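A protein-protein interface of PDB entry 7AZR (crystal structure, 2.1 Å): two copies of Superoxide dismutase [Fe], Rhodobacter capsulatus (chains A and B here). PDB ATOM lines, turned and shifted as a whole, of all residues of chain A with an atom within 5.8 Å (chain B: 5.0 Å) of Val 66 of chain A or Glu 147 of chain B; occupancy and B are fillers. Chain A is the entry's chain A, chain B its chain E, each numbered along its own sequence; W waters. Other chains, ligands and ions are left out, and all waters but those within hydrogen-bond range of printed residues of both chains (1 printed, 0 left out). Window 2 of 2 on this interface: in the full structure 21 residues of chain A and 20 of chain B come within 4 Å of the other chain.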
ATOM      1  N   GLY A  64     -13.819 -20.892 -10.466  1.00  0.00           N
ATOM      2  CA  GLY A  64     -13.588 -22.306 -10.718  1.00  0.00           C
ATOM      3  C   GLY A  64     -13.019 -22.625 -12.087  1.00  0.00           C
ATOM      4  O   GLY A  64     -12.611 -23.758 -12.318  1.00  0.00           O
ATOM      5  N   ALA A  65     -12.991 -21.636 -12.987  1.00  0.00           N
ATOM      6  CA  ALA A  65     -12.359 -21.825 -14.300  1.00  0.00           C
ATOM      7  C   ALA A  65     -10.874 -21.870 -14.109  1.00  0.00           C
ATOM      8  O   ALA A  65     -10.310 -21.121 -13.289  1.00  0.00           O
ATOM      9  CB  ALA A  65     -12.720 -20.726 -15.285  1.00  0.00           C
ATOM     10  N   VAL A  66     -10.225 -22.782 -14.848  1.00  0.00           N
ATOM     11  CA  VAL A  66      -8.786 -22.900 -14.838  1.00  0.00           C
ATOM     12  C   VAL A  66      -8.212 -21.701 -15.591  1.00  0.00           C
ATOM     13  O   VAL A  66      -7.264 -21.062 -15.151  1.00  0.00           O
ATOM     14  CB  VAL A  66      -8.327 -24.232 -15.487  1.00  0.00           C
ATOM     15  CG1 VAL A  66      -6.828 -24.340 -15.448  1.00  0.00           C
ATOM     16  CG2 VAL A  66      -8.955 -25.416 -14.763  1.00  0.00           C
ATOM     17  N   ALA A  67      -8.782 -21.421 -16.762  1.00  0.00           N
ATOM     18  CA  ALA A  67      -8.387 -20.298 -17.602  1.00  0.00           C
ATOM     19  C   ALA A  67      -9.529 -19.286 -17.589  1.00  0.00           C
ATOM     20  O   ALA A  67     -10.681 -19.679 -17.730  1.00  0.00           O
ATOM     21  CB  ALA A  67      -8.117 -20.769 -19.016  1.00  0.00           C
ATOM     22  N   GLN A  68      -9.185 -18.008 -17.359  1.00  0.00           N
ATOM     23  CA  GLN A  68     -10.144 -16.898 -17.333  1.00  0.00           C
ATOM     24  C   GLN A  68     -10.175 -16.276 -18.749  1.00  0.00           C
ATOM     25  O   GLN A  68      -9.352 -16.631 -19.582  1.00  0.00           O
ATOM     26  CB  GLN A  68      -9.683 -15.880 -16.298  1.00  0.00           C
ATOM     27  CG  GLN A  68      -9.519 -16.460 -14.898  1.00  0.00           C
ATOM     28  CD  GLN A  68     -10.840 -16.843 -14.229  1.00  0.00           C
ATOM     29  OE1 GLN A  68     -11.886 -16.237 -14.506  1.00  0.00           O
ATOM     30  NE2 GLN A  68     -10.790 -17.817 -13.300  1.00  0.00           N
ATOM     31  N   GLU A 147      -3.359 -17.587  -8.785  1.00  0.00           N
ATOM     32  CA  GLU A 147      -2.797 -17.865 -10.107  1.00  0.00           C
ATOM     33  C   GLU A 147      -2.949 -16.713 -11.080  1.00  0.00           C
ATOM     34  O   GLU A 147      -3.984 -16.037 -11.112  1.00  0.00           O
ATOM     35  CB  GLU A 147      -3.433 -19.115 -10.720  1.00  0.00           C
ATOM     36  CG  GLU A 147      -4.874 -19.024 -11.221  1.00  0.00           C
ATOM     37  CD  GLU A 147      -5.940 -19.133 -10.116  1.00  0.00           C
ATOM     38  OE1 GLU A 147      -5.579 -19.281  -8.909  1.00  0.00           O
ATOM     39  OE2 GLU A 147      -7.154 -19.081 -10.443  1.00  0.00           O
ATOM     40  N   ASN A 148      -1.913 -16.528 -11.903  1.00  0.00           N
ATOM     41  CA  ASN A 148      -1.971 -15.703 -13.088  1.00  0.00           C
ATOM     42  C   ASN A 148      -2.341 -14.249 -12.699  1.00  0.00           C
ATOM     43  O   ASN A 148      -1.564 -13.606 -11.995  1.00  0.00           O
ATOM     44  CB  ASN A 148      -2.902 -16.366 -14.108  1.00  0.00           C
ATOM     45  CG  ASN A 148      -2.479 -17.795 -14.416  1.00  0.00           C
ATOM     46  OD1 ASN A 148      -1.270 -18.094 -14.468  1.00  0.00           O
ATOM     47  ND2 ASN A 148      -3.460 -18.691 -14.605  1.00  0.00           N
ATOM     48  N   ALA B  65      -9.851 -29.407 -10.739  1.00  0.00           N
ATOM     49  CA  ALA B  65      -9.102 -28.525  -9.858  1.00  0.00           C
ATOM     50  C   ALA B  65      -8.290 -27.463 -10.584  1.00  0.00           C
ATOM     51  O   ALA B  65      -7.656 -27.726 -11.606  1.00  0.00           O
ATOM     52  CB  ALA B  65      -8.233 -29.328  -8.898  1.00  0.00           C
ATOM     53  N   VAL B  66      -8.328 -26.252 -10.022  1.00  0.00           N
ATOM     54  CA  VAL B  66      -7.587 -25.092 -10.506  1.00  0.00           C
ATOM     55  C   VAL B  66      -6.094 -25.326 -10.299  1.00  0.00           C
ATOM     56  O   VAL B  66      -5.304 -25.092 -11.174  1.00  0.00           O
ATOM     57  CB  VAL B  66      -8.084 -23.823  -9.763  1.00  0.00           C
ATOM     58  CG1 VAL B  66      -7.214 -22.602 -10.065  1.00  0.00           C
ATOM     59  CG2 VAL B  66      -9.519 -23.552 -10.158  1.00  0.00           C
ATOM     60  N   GLN B  68      -3.180 -28.249  -8.977  1.00  0.00           N
ATOM     61  CA  GLN B  68      -2.908 -29.671  -8.843  1.00  0.00           C
ATOM     62  C   GLN B  68      -2.075 -29.896  -7.591  1.00  0.00           C
ATOM     63  O   GLN B  68      -1.571 -28.938  -7.029  1.00  0.00           O
ATOM     64  CB  GLN B  68      -2.183 -30.160 -10.097  1.00  0.00           C
ATOM     65  CG  GLN B  68      -2.903 -29.868 -11.409  1.00  0.00           C
ATOM     66  CD  GLN B  68      -4.236 -30.627 -11.525  1.00  0.00           C
ATOM     67  OE1 GLN B  68      -4.387 -31.750 -11.002  1.00  0.00           O
ATOM     68  NE2 GLN B  68      -5.205 -30.013 -12.217  1.00  0.00           N
ATOM     69  N   GLN B 125      -1.348 -19.095 -24.086  1.00  0.00           N
ATOM     70  CA  GLN B 125      -1.415 -19.693 -22.758  1.00  0.00           C
ATOM     71  C   GLN B 125      -1.052 -18.622 -21.746  1.00  0.00           C
ATOM     72  O   GLN B 125       0.116 -18.267 -21.605  1.00  0.00           O
ATOM     73  CB  GLN B 125      -0.500 -20.894 -22.609  1.00  0.00           C
ATOM     74  CG  GLN B 125      -0.615 -21.613 -21.273  1.00  0.00           C
ATOM     75  CD  GLN B 125      -1.989 -22.176 -21.014  1.00  0.00           C
ATOM     76  OE1 GLN B 125      -2.623 -22.704 -21.932  1.00  0.00           O
ATOM     77  NE2 GLN B 125      -2.479 -22.041 -19.775  1.00  0.00           N
ATOM     78  N   SER B 128       2.015 -19.538 -17.064  1.00  0.00           N
ATOM     79  CA  SER B 128       2.982 -20.586 -17.311  1.00  0.00           C
ATOM     80  C   SER B 128       2.272 -21.781 -17.932  1.00  0.00           C
ATOM     81  O   SER B 128       1.117 -22.081 -17.583  1.00  0.00           O
ATOM     82  CB  SER B 128       3.621 -21.035 -15.985  1.00  0.00           C
ATOM     83  OG  SER B 128       4.239 -19.964 -15.314  1.00  0.00           O
ATOM     84  N   GLY B 129       2.982 -22.484 -18.822  1.00  0.00           N
ATOM     85  CA  GLY B 129       2.456 -23.702 -19.430  1.00  0.00           C
ATOM     86  C   GLY B 129       3.233 -24.149 -20.652  1.00  0.00           C
ATOM     87  O   GLY B 129       4.419 -23.856 -20.781  1.00  0.00           O
ATOM     88  N   LYS B 145      -2.912 -26.463 -25.736  1.00  0.00           N
ATOM     89  CA  LYS B 145      -2.122 -25.736 -24.775  1.00  0.00           C
ATOM     90  C   LYS B 145      -2.606 -26.092 -23.393  1.00  0.00           C
ATOM     91  O   LYS B 145      -3.755 -26.418 -23.213  1.00  0.00           O
ATOM     92  CB  LYS B 145      -2.213 -24.234 -25.025  1.00  0.00           C
ATOM     93  CG  LYS B 145      -3.621 -23.641 -25.058  1.00  0.00           C
ATOM     94  CD  LYS B 145      -3.488 -22.202 -25.494  1.00  0.00           C
ATOM     95  CE  LYS B 145      -4.584 -21.303 -25.019  1.00  0.00           C
ATOM     96  NZ  LYS B 145      -5.891 -21.723 -25.435  1.00  0.00           N
ATOM     97  N   THR B 146      -1.675 -26.093 -22.442  1.00  0.00           N
ATOM     98  CA  THR B 146      -1.923 -26.505 -21.087  1.00  0.00           C
ATOM     99  C   THR B 146      -1.241 -25.573 -20.104  1.00  0.00           C
ATOM    100  O   THR B 146      -0.247 -24.893 -20.455  1.00  0.00           O
ATOM    101  CB  THR B 146      -1.388 -27.928 -20.834  1.00  0.00           C
ATOM    102  OG1 THR B 146       0.019 -27.971 -21.115  1.00  0.00           O
ATOM    103  CG2 THR B 146      -2.163 -28.952 -21.675  1.00  0.00           C
ATOM    104  N   GLU B 147      -1.807 -25.515 -18.892  1.00  0.00           N
ATOM    105  CA  GLU B 147      -1.262 -24.747 -17.790  1.00  0.00           C
ATOM    106  C   GLU B 147      -0.206 -25.518 -16.981  1.00  0.00           C
ATOM    107  O   GLU B 147      -0.344 -26.715 -16.733  1.00  0.00           O
ATOM    108  CB  GLU B 147      -2.389 -24.302 -16.863  1.00  0.00           C
ATOM    109  CG  GLU B 147      -3.003 -25.332 -15.902  1.00  0.00           C
ATOM    110  CD  GLU B 147      -4.056 -26.257 -16.508  1.00  0.00           C
ATOM    111  OE1 GLU B 147      -4.226 -26.280 -17.738  1.00  0.00           O
ATOM    112  OE2 GLU B 147      -4.681 -27.010 -15.719  1.00  0.00           O
ATOM    113  N   ASN B 148       0.828 -24.791 -16.556  1.00  0.00           N
ATOM    114  CA  ASN B 148       1.748 -25.239 -15.538  1.00  0.00           C
ATOM    115  C   ASN B 148       2.449 -26.539 -15.984  1.00  0.00           C
ATOM    116  O   ASN B 148       3.192 -26.507 -16.967  1.00  0.00           O
ATOM    117  CB  ASN B 148       1.028 -25.299 -14.190  1.00  0.00           C
ATOM    118  CG  ASN B 148       0.384 -23.972 -13.848  1.00  0.00           C
ATOM    119  OD1 ASN B 148       0.976 -22.919 -14.121  1.00  0.00           O
ATOM    120  ND2 ASN B 148      -0.820 -23.995 -13.264  1.00  0.00           N
ATOM    121  N   GLY B 149       2.214 -27.649 -15.279  1.00  0.00           N
ATOM    122  CA  GLY B 149       2.725 -28.934 -15.682  1.00  0.00           C
ATOM    123  C   GLY B 149       1.766 -29.846 -16.439  1.00  0.00           C
ATOM    124  O   GLY B 149       2.195 -30.914 -16.946  1.00  0.00           O
ATOM    125  N   VAL B 150       0.499 -29.429 -16.559  1.00  0.00           N
ATOM    126  CA  VAL B 150      -0.504 -30.250 -17.257  1.00  0.00           C
ATOM    127  C   VAL B 150      -0.012 -30.538 -18.686  1.00  0.00           C
ATOM    128  O   VAL B 150       0.680 -29.729 -19.293  1.00  0.00           O
ATOM    129  CB  VAL B 150      -1.904 -29.614 -17.212  1.00  0.00           C
ATOM    130  CG1 VAL B 150      -2.889 -30.386 -18.059  1.00  0.00           C
ATOM    131  CG2 VAL B 150      -2.391 -29.518 -15.766  1.00  0.00           C
HETATM  132  O   HOH W   1       0.668 -20.089 -14.524  1.00  0.00           O
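Among the printed residues, pairs that only touch across the chains: Gly 64 of chain A with Val 66 of chain B, Val 66 of chain A with Glu 147 of chain B and Glu 147 of chain A with Val 66 of chain B.
Val 66 of chain A touches just one residue of chain B: Glu 147 (3.4 Å).
Printed residues of chain A within 4 Å of Glu 147 of chain B: Val 66.
Printed residues of chain B within 4 Å of Glu 147 of chain A: Val 66.
Of the printed residues of chain B, Gly 64 of chain A touches Val 66.
Of the printed residues of chain A, Val 66 of chain B touches Gly 64 (3.8 Å) and Glu 147 (3.5 Å).
Asn 148 of chain A touches none of the printed residues of chain B.
The nearest residue of chain B that does not touch Val 66 of chain A is Ala 65 of chain B (4.1 Å).
The nearest printed residue of chain A that does not touch Glu 147 of chain B is Asn 148 of chain A (6.1 Å).
Of the 12 printed residues of chain B, 2 touch a printed residue of chain A.
Of the 7 printed residues of chain A, 3 touch a printed residue of chain B.
Hydrophobic or aromatic side chains of chain A that line the printed part of chain B: Val 66.
Among the printed residues, no Asp or Glu carboxylate lies within 4 Å of a Lys or Arg side-chain nitrogen of the other chain.
Val 66 of chain A touches Glu 147 of chain B, and with the chains exchanged Glu 147 of chain A touches Val 66 of chain B.
Of the 3 pairs that touch across the chains among the printed residues, 2 have their exchanged pair printed and touching as well.
Water W1 lies within hydrogen-bond range of the side-chain amide oxygen (OD1) of Asn 148 of chain A (2.8 Å), the side-chain amide oxygen (OD1) of Asn 148 of chain B (2.9 Å) and the backbone NH (N) of Ser 128 of chain B (2.9 Å).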
